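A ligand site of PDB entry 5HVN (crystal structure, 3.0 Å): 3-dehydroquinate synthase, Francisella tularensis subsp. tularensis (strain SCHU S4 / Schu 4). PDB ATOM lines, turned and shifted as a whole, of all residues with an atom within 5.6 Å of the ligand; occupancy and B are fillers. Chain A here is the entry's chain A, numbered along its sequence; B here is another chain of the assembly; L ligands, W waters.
The backbone carbonyl oxygen (O) of Thr 132 sits at hydrogen-bond distance from a nitrogen (N3) of the ligand, at 2.8 Å.
The side-chain hydroxyl (OG1) of Thr 132 is in hydrogen-bond range of a nitrogen (N2) of the ligand, at 2.6 Å.
The side-chain carboxylate of Glu 75 sits at hydrogen-bond distance from an oxygen (O12) of the ligand, 2.6 Å away.
The side-chain carboxylate (OD2) of Asp 73 lies within hydrogen-bond range of an oxygen (O6) of the ligand (2.7 Å).
N of Gly 108 sits at hydrogen-bond distance from O9 of the ligand (2.7 Å).
OG1 of Thr 175 lies within hydrogen-bond range of N4 of the ligand, 2.8 Å away.
The side-chain hydroxyl (OG1) of Thr 133 is in hydrogen-bond range of an oxygen (O9) of the ligand.
An oxygen (O1) of the ligand is in hydrogen-bond range of the backbone NH (N) of Val 109 (2.8 Å).
An oxygen (O6) of the ligand sits at hydrogen-bond distance from the side-chain amide nitrogen of Asn 45 (2.8 Å).
The backbone carbonyl oxygen (O) of Lys 145 sits at hydrogen-bond distance from a nitrogen (N7) of the ligand.
O13 of the ligand lies within hydrogen-bond range of NZ of Lys 78, at 2.9 Å.
OD1 of Asp 112 lies close to N7 of the ligand (3.3 Å).
N3 of the ligand lies within hydrogen-bond range of O of Phe 172, 3.2 Å away.
The backbone NH of Leu 176 sits at hydrogen-bond distance from a nitrogen (N4) of the ligand (3.4 Å).
N of Thr 132 sits at hydrogen-bond distance from O of Gly 106, at 2.8 Å.
The side-chain carboxylate of Asp 73 lies within hydrogen-bond range of the side-chain hydroxyl of Thr 47 (2.8 Å).
The side-chain hydroxyl (OG1) of Thr 175 sits at hydrogen-bond distance from the backbone carbonyl oxygen (O) of Phe 172 (3.3 Å).
The side-chain hydroxyl (OH) of Tyr 52 lies within hydrogen-bond range of the side-chain hydroxyl (OG1) of Thr 175 (2.6 Å).
The side-chain amino group (NZ) of Lys 78 lies within salt-bridge range of the side-chain carboxylate (OD2) of Asp 112 (3.0 Å).
The side-chain amide oxygen of Asn 155 lies within hydrogen-bond range of the side-chain amino group of Lys 78.
The side-chain amino group (NZ) of Lys 228 is in salt-bridge range of the side-chain carboxylate (OD1) of Asp 139 (2.9 Å).
The backbone carbonyl oxygen (O) of Val 142 is in hydrogen-bond range of the side-chain amino group (NZ) of Lys 228 (3.1 Å).
O of Asp 139 sits close to O14 of the ligand (3.4 Å).
Merely in contact with the ligand: Gly 107 (3.2 Å), Glu 180 (3.5 Å), Thr 47 (3.5 Å), Leu 51 (3.5 Å), Asn 155 (3.5 Å), Leu 135 (3.6 Å), Tyr 52 (3.7 Å), Ser 140 (3.7 Å), Val 48 (3.8 Å), Lys 228 (3.9 Å) and Pro 177 (3.98 Å).
Hydrophobic or aromatic side chains within 4 Å of the ligand: Val 48, Leu 51, Tyr 52, Val 109, Leu 135, Phe 172, Leu 176 and Pro 177.
Within 4 Å of the ligand: Asn 45, Thr 47, Val 48, Leu 51, Tyr 52, Asp 73, Glu 75, Lys 78, Gly 107, Gly 108, Val 109, Asp 112, Thr 132, Thr 133, Leu 135, Asp 139, Ser 140, Lys 145, Asn 155, Phe 172, Thr 175, Leu 176, Pro 177, Glu 180 and Lys 228.
Along chain A the residues within 4 Å of the ligand span positions 45 to 228.
The nearest printed residue that does not touch the ligand is Ser 136 (4.1 Å).
Water W1 lies within hydrogen-bond range of N of Gly 107 (2.7 Å), O1 of the ligand (2.8 Å) and N of Ile 110 (3.4 Å).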
ATOM      1  N   ASN A  45      -3.713   2.496  28.299  1.00  0.00           N
ATOM      2  CA  ASN A  45      -3.291   3.763  27.739  1.00  0.00           C
ATOM      3  C   ASN A  45      -4.009   4.833  28.591  1.00  0.00           C
ATOM      4  O   ASN A  45      -4.854   4.503  29.428  1.00  0.00           O
ATOM      5  CB  ASN A  45      -3.578   3.876  26.245  1.00  0.00           C
ATOM      6  CG  ASN A  45      -5.058   3.804  25.901  1.00  0.00           C
ATOM      7  OD1 ASN A  45      -5.940   4.111  26.723  1.00  0.00           O
ATOM      8  ND2 ASN A  45      -5.331   3.396  24.658  1.00  0.00           N
ATOM      9  N   THR A  47      -6.388   7.006  27.957  1.00  0.00           N
ATOM     10  CA  THR A  47      -7.848   7.040  27.810  1.00  0.00           C
ATOM     11  C   THR A  47      -8.569   5.925  28.570  1.00  0.00           C
ATOM     12  O   THR A  47      -9.452   6.182  29.397  1.00  0.00           O
ATOM     13  CB  THR A  47      -8.253   6.987  26.325  1.00  0.00           C
ATOM     14  OG1 THR A  47      -7.596   8.021  25.604  1.00  0.00           O
ATOM     15  CG2 THR A  47      -9.737   7.183  26.185  1.00  0.00           C
ATOM     16  N   VAL A  48      -8.207   4.674  28.272  1.00  0.00           N
ATOM     17  CA  VAL A  48      -8.847   3.541  28.924  1.00  0.00           C
ATOM     18  C   VAL A  48      -8.651   3.637  30.439  1.00  0.00           C
ATOM     19  O   VAL A  48      -9.534   3.260  31.215  1.00  0.00           O
ATOM     20  CB  VAL A  48      -8.361   2.198  28.329  1.00  0.00           C
ATOM     21  CG1 VAL A  48      -9.111   1.024  28.936  1.00  0.00           C
ATOM     22  CG2 VAL A  48      -8.582   2.194  26.839  1.00  0.00           C
ATOM     23  N   LEU A  51     -11.118   6.161  32.087  1.00  0.00           N
ATOM     24  CA  LEU A  51     -12.459   5.589  32.140  1.00  0.00           C
ATOM     25  C   LEU A  51     -12.636   4.360  32.983  1.00  0.00           C
ATOM     26  O   LEU A  51     -13.679   4.212  33.648  1.00  0.00           O
ATOM     27  CB  LEU A  51     -12.899   5.229  30.707  1.00  0.00           C
ATOM     28  CG  LEU A  51     -12.921   6.338  29.648  1.00  0.00           C
ATOM     29  CD1 LEU A  51     -13.031   5.739  28.259  1.00  0.00           C
ATOM     30  CD2 LEU A  51     -14.017   7.352  29.950  1.00  0.00           C
ATOM     31  N   TYR A  52     -11.645   3.464  32.983  1.00  0.00           N
ATOM     32  CA  TYR A  52     -11.791   2.210  33.733  1.00  0.00           C
ATOM     33  C   TYR A  52     -10.783   1.813  34.793  1.00  0.00           C
ATOM     34  O   TYR A  52     -11.090   0.956  35.627  1.00  0.00           O
ATOM     35  CB  TYR A  52     -11.922   1.051  32.735  1.00  0.00           C
ATOM     36  CG  TYR A  52     -13.052   1.222  31.774  1.00  0.00           C
ATOM     37  CD1 TYR A  52     -14.372   0.892  32.160  1.00  0.00           C
ATOM     38  CD2 TYR A  52     -12.841   1.714  30.467  1.00  0.00           C
ATOM     39  CE1 TYR A  52     -15.429   1.040  31.280  1.00  0.00           C
ATOM     40  CE2 TYR A  52     -13.903   1.870  29.583  1.00  0.00           C
ATOM     41  CZ  TYR A  52     -15.192   1.522  30.003  1.00  0.00           C
ATOM     42  OH  TYR A  52     -16.256   1.651  29.154  1.00  0.00           O
ATOM     43  N   ASP A  73      -1.854   6.918  24.366  1.00  0.00           N
ATOM     44  CA  ASP A  73      -2.845   6.485  23.420  1.00  0.00           C
ATOM     45  C   ASP A  73      -2.350   6.622  21.982  1.00  0.00           C
ATOM     46  O   ASP A  73      -1.868   7.672  21.582  1.00  0.00           O
ATOM     47  CB  ASP A  73      -4.155   7.230  23.655  1.00  0.00           C
ATOM     48  CG  ASP A  73      -5.320   6.547  23.026  1.00  0.00           C
ATOM     49  OD1 ASP A  73      -5.052   5.537  22.331  1.00  0.00           O
ATOM     50  OD2 ASP A  73      -6.487   6.971  23.216  1.00  0.00           O
ATOM     51  N   GLY A  74      -2.451   5.548  21.208  1.00  0.00           N
ATOM     52  CA  GLY A  74      -1.999   5.596  19.850  1.00  0.00           C
ATOM     53  C   GLY A  74      -1.174   4.425  19.375  1.00  0.00           C
ATOM     54  O   GLY A  74      -0.374   3.868  20.124  1.00  0.00           O
ATOM     55  N   GLU A  75      -1.377   4.090  18.096  1.00  0.00           N
ATOM     56  CA  GLU A  75      -0.704   3.012  17.388  1.00  0.00           C
ATOM     57  C   GLU A  75       0.807   3.243  17.397  1.00  0.00           C
ATOM     58  O   GLU A  75       1.586   2.278  17.470  1.00  0.00           O
ATOM     59  CB  GLU A  75      -1.233   2.968  15.955  1.00  0.00           C
ATOM     60  CG  GLU A  75      -0.612   1.905  15.058  1.00  0.00           C
ATOM     61  CD  GLU A  75      -1.056   0.517  15.422  1.00  0.00           C
ATOM     62  OE1 GLU A  75      -2.218   0.387  15.895  1.00  0.00           O
ATOM     63  OE2 GLU A  75      -0.272  -0.449  15.187  1.00  0.00           O
ATOM     64  N   LYS A  78       2.859   1.474  20.131  1.00  0.00           N
ATOM     65  CA  LYS A  78       2.971   0.009  20.184  1.00  0.00           C
ATOM     66  C   LYS A  78       4.393  -0.188  19.633  1.00  0.00           C
ATOM     67  O   LYS A  78       4.632  -0.808  18.589  1.00  0.00           O
ATOM     68  CB  LYS A  78       1.879  -0.583  19.305  1.00  0.00           C
ATOM     69  CG  LYS A  78       1.787  -2.080  19.195  1.00  0.00           C
ATOM     70  CD  LYS A  78       0.663  -2.342  18.207  1.00  0.00           C
ATOM     71  CE  LYS A  78       0.788  -3.705  17.573  1.00  0.00           C
ATOM     72  NZ  LYS A  78      -0.361  -3.931  16.668  1.00  0.00           N
ATOM     73  N   GLY A 106      -7.485  -2.569  27.683  1.00  0.00           N
ATOM     74  CA  GLY A 106      -7.549  -1.613  26.593  1.00  0.00           C
ATOM     75  C   GLY A 106      -7.952  -2.282  25.291  1.00  0.00           C
ATOM     76  O   GLY A 106      -8.504  -3.388  25.290  1.00  0.00           O
ATOM     77  N   GLY A 107      -7.685  -1.611  24.175  1.00  0.00           N
ATOM     78  CA  GLY A 107      -8.019  -2.169  22.874  1.00  0.00           C
ATOM     79  C   GLY A 107      -6.872  -2.968  22.291  1.00  0.00           C
ATOM     80  O   GLY A 107      -5.895  -3.277  22.969  1.00  0.00           O
ATOM     81  N   GLY A 108      -7.006  -3.293  21.013  1.00  0.00           N
ATOM     82  CA  GLY A 108      -6.014  -4.037  20.275  1.00  0.00           C
ATOM     83  C   GLY A 108      -4.561  -3.623  20.457  1.00  0.00           C
ATOM     84  O   GLY A 108      -3.688  -4.488  20.563  1.00  0.00           O
ATOM     85  N   VAL A 109      -4.274  -2.314  20.473  1.00  0.00           N
ATOM     86  CA  VAL A 109      -2.882  -1.863  20.631  1.00  0.00           C
ATOM     87  C   VAL A 109      -2.310  -2.340  21.963  1.00  0.00           C
ATOM     88  O   VAL A 109      -1.244  -2.960  21.992  1.00  0.00           O
ATOM     89  CB  VAL A 109      -2.731  -0.346  20.461  1.00  0.00           C
ATOM     90  CG1 VAL A 109      -1.360   0.130  20.917  1.00  0.00           C
ATOM     91  CG2 VAL A 109      -2.951   0.031  19.017  1.00  0.00           C
ATOM     92  N   ILE A 110      -3.053  -2.087  23.051  1.00  0.00           N
ATOM     93  CA  ILE A 110      -2.664  -2.526  24.380  1.00  0.00           C
ATOM     94  C   ILE A 110      -2.579  -4.052  24.419  1.00  0.00           C
ATOM     95  O   ILE A 110      -1.647  -4.589  25.000  1.00  0.00           O
ATOM     96  CB  ILE A 110      -3.616  -1.966  25.459  1.00  0.00           C
ATOM     97  CG1 ILE A 110      -3.376  -0.448  25.629  1.00  0.00           C
ATOM     98  CG2 ILE A 110      -3.451  -2.691  26.804  1.00  0.00           C
ATOM     99  CD1 ILE A 110      -1.949  -0.088  25.967  1.00  0.00           C
ATOM    100  N   ASP A 112      -1.823  -6.172  21.999  1.00  0.00           N
ATOM    101  CA  ASP A 112      -0.664  -6.677  21.294  1.00  0.00           C
ATOM    102  C   ASP A 112       0.603  -6.556  22.060  1.00  0.00           C
ATOM    103  O   ASP A 112       1.359  -7.538  22.168  1.00  0.00           O
ATOM    104  CB  ASP A 112      -0.478  -6.012  19.917  1.00  0.00           C
ATOM    105  CG  ASP A 112      -1.340  -6.630  18.833  1.00  0.00           C
ATOM    106  OD1 ASP A 112      -2.507  -6.998  19.096  1.00  0.00           O
ATOM    107  OD2 ASP A 112      -0.834  -6.725  17.689  1.00  0.00           O
ATOM    108  N   THR A 132     -11.279  -3.704  25.278  1.00  0.00           N
ATOM    109  CA  THR A 132     -12.268  -2.652  25.549  1.00  0.00           C
ATOM    110  C   THR A 132     -12.848  -2.020  24.283  1.00  0.00           C
ATOM    111  O   THR A 132     -13.554  -0.996  24.347  1.00  0.00           O
ATOM    112  CB  THR A 132     -11.731  -1.570  26.504  1.00  0.00           C
ATOM    113  OG1 THR A 132     -10.674  -0.849  25.870  1.00  0.00           O
ATOM    114  CG2 THR A 132     -11.257  -2.188  27.838  1.00  0.00           C
ATOM    115  N   THR A 133     -12.550  -2.632  23.142  1.00  0.00           N
ATOM    116  CA  THR A 133     -13.065  -2.177  21.854  1.00  0.00           C
ATOM    117  C   THR A 133     -13.675  -3.392  21.174  1.00  0.00           C
ATOM    118  O   THR A 133     -13.198  -4.524  21.361  1.00  0.00           O
ATOM    119  CB  THR A 133     -11.949  -1.666  20.931  1.00  0.00           C
ATOM    120  OG1 THR A 133     -11.047  -2.735  20.600  1.00  0.00           O
ATOM    121  CG2 THR A 133     -11.193  -0.514  21.540  1.00  0.00           C
ATOM    122  N   LEU A 135     -13.528  -4.267  18.052  1.00  0.00           N
ATOM    123  CA  LEU A 135     -12.554  -4.913  17.191  1.00  0.00           C
ATOM    124  C   LEU A 135     -11.662  -5.856  17.991  1.00  0.00           C
ATOM    125  O   LEU A 135     -11.501  -7.013  17.593  1.00  0.00           O
ATOM    126  CB  LEU A 135     -11.757  -3.914  16.384  1.00  0.00           C
ATOM    127  CG  LEU A 135     -10.781  -4.448  15.331  1.00  0.00           C
ATOM    128  CD1 LEU A 135     -10.433  -3.308  14.397  1.00  0.00           C
ATOM    129  CD2 LEU A 135      -9.522  -5.038  15.913  1.00  0.00           C
ATOM    130  N   SER A 136     -11.109  -5.406  19.124  1.00  0.00           N
ATOM    131  CA  SER A 136     -10.258  -6.292  19.915  1.00  0.00           C
ATOM    132  C   SER A 136     -11.044  -7.452  20.561  1.00  0.00           C
ATOM    133  O   SER A 136     -10.479  -8.502  20.813  1.00  0.00           O
ATOM    134  CB  SER A 136      -9.430  -5.548  20.953  1.00  0.00           C
ATOM    135  OG  SER A 136     -10.270  -4.851  21.844  1.00  0.00           O
ATOM    136  N   ASP A 139     -11.358  -9.967  17.536  1.00  0.00           N
ATOM    137  CA  ASP A 139     -10.174 -10.279  16.756  1.00  0.00           C
ATOM    138  C   ASP A 139      -8.922 -10.663  17.590  1.00  0.00           C
ATOM    139  O   ASP A 139      -8.264 -11.655  17.272  1.00  0.00           O
ATOM    140  CB  ASP A 139      -9.916  -9.133  15.800  1.00  0.00           C
ATOM    141  CG  ASP A 139      -9.449  -9.589  14.446  1.00  0.00           C
ATOM    142  OD1 ASP A 139      -8.728 -10.626  14.314  1.00  0.00           O
ATOM    143  OD2 ASP A 139      -9.813  -8.892  13.493  1.00  0.00           O
ATOM    144  N   SER A 140      -8.615  -9.903  18.648  1.00  0.00           N
ATOM    145  CA  SER A 140      -7.481 -10.178  19.558  1.00  0.00           C
ATOM    146  C   SER A 140      -7.703 -11.373  20.520  1.00  0.00           C
ATOM    147  O   SER A 140      -6.761 -12.041  20.915  1.00  0.00           O
ATOM    148  CB  SER A 140      -7.236  -8.964  20.451  1.00  0.00           C
ATOM    149  OG  SER A 140      -7.014  -7.779  19.714  1.00  0.00           O
ATOM    150  N   VAL A 142      -8.701 -14.346  20.145  1.00  0.00           N
ATOM    151  CA  VAL A 142      -8.424 -15.689  19.562  1.00  0.00           C
ATOM    152  C   VAL A 142      -7.281 -15.603  18.555  1.00  0.00           C
ATOM    153  O   VAL A 142      -7.130 -14.607  17.855  1.00  0.00           O
ATOM    154  CB  VAL A 142      -9.672 -16.242  18.816  1.00  0.00           C
ATOM    155  CG1 VAL A 142      -9.368 -17.527  18.056  1.00  0.00           C
ATOM    156  CG2 VAL A 142     -10.833 -16.457  19.777  1.00  0.00           C
ATOM    157  N   LYS A 145      -1.956 -14.057  18.321  1.00  0.00           N
ATOM    158  CA  LYS A 145      -0.995 -13.079  17.786  1.00  0.00           C
ATOM    159  C   LYS A 145      -0.724 -11.911  18.715  1.00  0.00           C
ATOM    160  O   LYS A 145      -1.643 -11.289  19.246  1.00  0.00           O
ATOM    161  CB  LYS A 145      -1.373 -12.580  16.391  1.00  0.00           C
ATOM    162  CG  LYS A 145      -1.275 -13.665  15.337  1.00  0.00           C
ATOM    163  CD  LYS A 145      -1.526 -13.129  13.940  1.00  0.00           C
ATOM    164  CE  LYS A 145      -1.404 -14.253  12.908  1.00  0.00           C
ATOM    165  NZ  LYS A 145      -1.453 -13.743  11.509  1.00  0.00           N
ATOM    166  N   THR A 146       0.548 -11.651  18.957  1.00  0.00           N
ATOM    167  CA  THR A 146       0.972 -10.521  19.762  1.00  0.00           C
ATOM    168  C   THR A 146       2.083  -9.913  18.913  1.00  0.00           C
ATOM    169  O   THR A 146       2.761 -10.670  18.174  1.00  0.00           O
ATOM    170  CB  THR A 146       1.530 -10.915  21.144  1.00  0.00           C
ATOM    171  OG1 THR A 146       2.859 -11.442  21.031  1.00  0.00           O
ATOM    172  CG2 THR A 146       0.614 -11.922  21.836  1.00  0.00           C
ATOM    173  N   ASN A 155       3.855  -4.406  13.019  1.00  0.00           N
ATOM    174  CA  ASN A 155       3.642  -5.802  13.410  1.00  0.00           C
ATOM    175  C   ASN A 155       4.672  -6.780  12.868  1.00  0.00           C
ATOM    176  O   ASN A 155       4.321  -7.869  12.446  1.00  0.00           O
ATOM    177  CB  ASN A 155       2.223  -6.278  13.086  1.00  0.00           C
ATOM    178  CG  ASN A 155       1.176  -5.605  13.951  1.00  0.00           C
ATOM    179  OD1 ASN A 155       1.126  -4.393  14.062  1.00  0.00           O
ATOM    180  ND2 ASN A 155       0.312  -6.401  14.564  1.00  0.00           N
ATOM    181  N   PHE A 172     -18.427  -1.699  27.775  1.00  0.00           N
ATOM    182  CA  PHE A 172     -17.355  -0.893  27.179  1.00  0.00           C
ATOM    183  C   PHE A 172     -17.826  -0.045  25.993  1.00  0.00           C
ATOM    184  O   PHE A 172     -17.215   1.002  25.701  1.00  0.00           O
ATOM    185  CB  PHE A 172     -16.180  -1.761  26.740  1.00  0.00           C
ATOM    186  CG  PHE A 172     -15.451  -2.418  27.858  1.00  0.00           C
ATOM    187  CD1 PHE A 172     -15.065  -1.689  29.000  1.00  0.00           C
ATOM    188  CD2 PHE A 172     -15.045  -3.760  27.756  1.00  0.00           C
ATOM    189  CE1 PHE A 172     -14.357  -2.289  30.030  1.00  0.00           C
ATOM    190  CE2 PHE A 172     -14.334  -4.361  28.777  1.00  0.00           C
ATOM    191  CZ  PHE A 172     -13.990  -3.625  29.914  1.00  0.00           C
ATOM    192  N   TYR A 173     -18.903  -0.465  25.334  1.00  0.00           N
ATOM    193  CA  TYR A 173     -19.413   0.284  24.197  1.00  0.00           C
ATOM    194  C   TYR A 173     -20.005   1.616  24.640  1.00  0.00           C
ATOM    195  O   TYR A 173     -20.131   2.530  23.810  1.00  0.00           O
ATOM    196  CB  TYR A 173     -20.450  -0.486  23.388  1.00  0.00           C
ATOM    197  CG  TYR A 173     -20.088  -1.898  23.022  1.00  0.00           C
ATOM    198  CD1 TYR A 173     -18.808  -2.219  22.541  1.00  0.00           C
ATOM    199  CD2 TYR A 173     -21.054  -2.920  23.071  1.00  0.00           C
ATOM    200  CE1 TYR A 173     -18.484  -3.516  22.183  1.00  0.00           C
ATOM    201  CE2 TYR A 173     -20.735  -4.224  22.701  1.00  0.00           C
ATOM    202  CZ  TYR A 173     -19.458  -4.521  22.259  1.00  0.00           C
ATOM    203  OH  TYR A 173     -19.134  -5.818  21.900  1.00  0.00           O
ATOM    204  N   THR A 175     -18.716   3.949  26.320  1.00  0.00           N
ATOM    205  CA  THR A 175     -17.710   5.007  26.260  1.00  0.00           C
ATOM    206  C   THR A 175     -16.941   5.011  24.952  1.00  0.00           C
ATOM    207  O   THR A 175     -16.189   5.951  24.689  1.00  0.00           O
ATOM    208  CB  THR A 175     -16.685   4.920  27.421  1.00  0.00           C
ATOM    209  OG1 THR A 175     -16.051   3.623  27.403  1.00  0.00           O
ATOM    210  CG2 THR A 175     -17.359   5.160  28.779  1.00  0.00           C
ATOM    211  N   LEU A 176     -17.133   3.971  24.133  1.00  0.00           N
ATOM    212  CA  LEU A 176     -16.453   3.805  22.833  1.00  0.00           C
ATOM    213  C   LEU A 176     -17.092   4.678  21.766  1.00  0.00           C
ATOM    214  O   LEU A 176     -18.299   4.564  21.489  1.00  0.00           O
ATOM    215  CB  LEU A 176     -16.501   2.343  22.406  1.00  0.00           C
ATOM    216  CG  LEU A 176     -15.643   1.908  21.217  1.00  0.00           C
ATOM    217  CD1 LEU A 176     -14.174   2.097  21.556  1.00  0.00           C
ATOM    218  CD2 LEU A 176     -15.877   0.447  20.905  1.00  0.00           C
ATOM    219  N   PRO A 177     -16.280   5.548  21.138  1.00  0.00           N
ATOM    220  CA  PRO A 177     -16.730   6.462  20.068  1.00  0.00           C
ATOM    221  C   PRO A 177     -17.397   5.729  18.925  1.00  0.00           C
ATOM    222  O   PRO A 177     -16.971   4.624  18.593  1.00  0.00           O
ATOM    223  CB  PRO A 177     -15.415   7.082  19.586  1.00  0.00           C
ATOM    224  CG  PRO A 177     -14.613   7.143  20.814  1.00  0.00           C
ATOM    225  CD  PRO A 177     -14.864   5.803  21.484  1.00  0.00           C
ATOM    226  N   GLU A 180     -15.087   4.175  16.303  1.00  0.00           N
ATOM    227  CA  GLU A 180     -14.385   2.999  16.796  1.00  0.00           C
ATOM    228  C   GLU A 180     -15.291   1.773  16.823  1.00  0.00           C
ATOM    229  O   GLU A 180     -14.860   0.691  16.405  1.00  0.00           O
ATOM    230  CB  GLU A 180     -13.685   3.255  18.138  1.00  0.00           C
ATOM    231  CG  GLU A 180     -12.386   4.036  17.974  1.00  0.00           C
ATOM    232  CD  GLU A 180     -11.311   3.247  17.195  1.00  0.00           C
ATOM    233  OE1 GLU A 180     -11.457   1.995  17.062  1.00  0.00           O
ATOM    234  OE2 GLU A 180     -10.307   3.871  16.754  1.00  0.00           O
ATOM    235  N   LYS A 228     -13.559 -17.437  14.354  1.00  0.00           N
ATOM    236  CA  LYS A 228     -12.105 -17.308  14.291  1.00  0.00           C
ATOM    237  C   LYS A 228     -11.419 -18.540  14.911  1.00  0.00           C
ATOM    238  O   LYS A 228     -10.383 -19.008  14.415  1.00  0.00           O
ATOM    239  CB  LYS A 228     -11.605 -16.025  14.946  1.00  0.00           C
ATOM    240  CG  LYS A 228     -10.113 -15.859  14.732  1.00  0.00           C
ATOM    241  CD  LYS A 228      -9.530 -14.568  15.246  1.00  0.00           C
ATOM    242  CE  LYS A 228      -8.101 -14.477  14.752  1.00  0.00           C
ATOM    243  NZ  LYS A 228      -7.521 -13.172  15.093  1.00  0.00           N
ATOM    244  N   HIS A 267      -8.032   1.414  11.587  1.00  0.00           N
ATOM    245  CA  HIS A 267      -7.762   0.056  11.121  1.00  0.00           C
ATOM    246  C   HIS A 267      -9.014  -0.657  10.614  1.00  0.00           C
ATOM    247  O   HIS A 267      -9.044  -1.150   9.485  1.00  0.00           O
ATOM    248  CB  HIS A 267      -7.066  -0.754  12.222  1.00  0.00           C
ATOM    249  CG  HIS A 267      -6.846  -2.191  11.884  1.00  0.00           C
ATOM    250  ND1 HIS A 267      -5.918  -2.604  10.951  1.00  0.00           N
ATOM    251  CD2 HIS A 267      -7.407  -3.323  12.383  1.00  0.00           C
ATOM    252  CE1 HIS A 267      -5.934  -3.925  10.871  1.00  0.00           C
ATOM    253  NE2 HIS A 267      -6.843  -4.380  11.731  1.00  0.00           N
ATOM    254  N   ARG B 123       7.238 -13.246  14.260  1.00  0.00           N
ATOM    255  CA  ARG B 123       6.836 -14.307  15.167  1.00  0.00           C
ATOM    256  C   ARG B 123       7.529 -15.640  14.886  1.00  0.00           C
ATOM    257  O   ARG B 123       6.903 -16.687  14.992  1.00  0.00           O
ATOM    258  CB  ARG B 123       5.323 -14.487  15.162  1.00  0.00           C
ATOM    259  CG  ARG B 123       4.571 -13.208  15.439  1.00  0.00           C
ATOM    260  CD  ARG B 123       3.070 -13.436  15.528  1.00  0.00           C
ATOM    261  NE  ARG B 123       2.374 -12.166  15.666  1.00  0.00           N
ATOM    262  CZ  ARG B 123       1.933 -11.445  14.641  1.00  0.00           C
ATOM    263  NH1 ARG B 123       2.114 -11.892  13.410  1.00  0.00           N
ATOM    264  NH2 ARG B 123       1.312 -10.293  14.838  1.00  0.00           N
HETATM  265  P1  LIG L   1      -6.864   0.732  19.505  1.00  0.00           P
HETATM  266  O1  LIG L   1      -6.367  -0.408  20.370  1.00  0.00           O
HETATM  267  O2  LIG L   1      -5.897   1.808  19.100  1.00  0.00           O
HETATM  268  O3  LIG L   1      -8.089   1.491  20.204  1.00  0.00           O
HETATM  269  C1  LIG L   1      -8.665   2.611  19.547  1.00  0.00           C
HETATM  270  C2  LIG L   1      -8.977   3.788  20.454  1.00  0.00           C
HETATM  271  O4  LIG L   1     -10.058   3.500  21.333  1.00  0.00           O
HETATM  272  C3  LIG L   1      -7.836   4.230  21.345  1.00  0.00           C
HETATM  273  O5  LIG L   1      -7.785   5.658  21.224  1.00  0.00           O
HETATM  274  C4  LIG L   1      -8.231   3.773  22.755  1.00  0.00           C
HETATM  275  O6  LIG L   1      -7.721   4.654  23.765  1.00  0.00           O
HETATM  276  C5  LIG L   1      -9.730   3.882  22.683  1.00  0.00           C
HETATM  277  N1  LIG L   1     -10.560   2.966  23.470  1.00  0.00           N
HETATM  278  C6  LIG L   1     -10.416   1.635  23.594  1.00  0.00           C
HETATM  279  N2  LIG L   1     -11.421   1.111  24.333  1.00  0.00           N
HETATM  280  C7  LIG L   1     -12.244   2.110  24.667  1.00  0.00           C
HETATM  281  C8  LIG L   1     -13.494   2.246  25.433  1.00  0.00           C
HETATM  282  N3  LIG L   1     -14.071   1.162  25.995  1.00  0.00           N
HETATM  283  N4  LIG L   1     -14.027   3.480  25.545  1.00  0.00           N
HETATM  284  C9  LIG L   1     -13.445   4.555  24.986  1.00  0.00           C
HETATM  285  N5  LIG L   1     -12.310   4.499  24.278  1.00  0.00           N
HETATM  286  C10 LIG L   1     -11.672   3.323  24.090  1.00  0.00           C
HETATM  287  O7  LIG L   1      -7.533   0.092  18.192  1.00  0.00           O
HETATM  288  P2  LIG L   1      -8.306  -1.313  18.093  1.00  0.00           P
HETATM  289  O8  LIG L   1      -9.412  -1.141  17.086  1.00  0.00           O
HETATM  290  O9  LIG L   1      -8.662  -1.821  19.458  1.00  0.00           O
HETATM  291  O10 LIG L   1      -7.206  -2.300  17.459  1.00  0.00           O
HETATM  292  C11 LIG L   1      -6.149  -1.788  16.655  1.00  0.00           C
HETATM  293  C12 LIG L   1      -4.887  -2.611  16.880  1.00  0.00           C
HETATM  294  O11 LIG L   1      -5.234  -3.967  17.177  1.00  0.00           O
HETATM  295  C13 LIG L   1      -4.006  -2.643  15.646  1.00  0.00           C
HETATM  296  O12 LIG L   1      -2.715  -2.165  16.010  1.00  0.00           O
HETATM  297  C14 LIG L   1      -3.932  -4.102  15.239  1.00  0.00           C
HETATM  298  O13 LIG L   1      -2.610  -4.476  14.852  1.00  0.00           O
HETATM  299  C15 LIG L   1      -4.362  -4.855  16.477  1.00  0.00           C
HETATM  300  N6  LIG L   1      -5.025  -6.130  16.168  1.00  0.00           N
HETATM  301  C16 LIG L   1      -4.464  -7.264  16.629  1.00  0.00           C
HETATM  302  C17 LIG L   1      -5.034  -8.509  16.370  1.00  0.00           C
HETATM  303  C18 LIG L   1      -4.377  -9.755  16.897  1.00  0.00           C
HETATM  304  O14 LIG L   1      -4.993 -10.800  16.910  1.00  0.00           O
HETATM  305  N7  LIG L   1      -3.122  -9.691  17.335  1.00  0.00           N
HETATM  306  C19 LIG L   1      -6.209  -8.586  15.621  1.00  0.00           C
HETATM  307  C20 LIG L   1      -6.785  -7.400  15.160  1.00  0.00           C
HETATM  308  C21 LIG L   1      -6.163  -6.184  15.450  1.00  0.00           C
HETATM  309  O   HOH W   1      -5.763  -0.006  23.109  1.00  0.00           O
HETATM  310  O   HOH W   2      -9.321   7.642  20.157  1.00  0.00           O
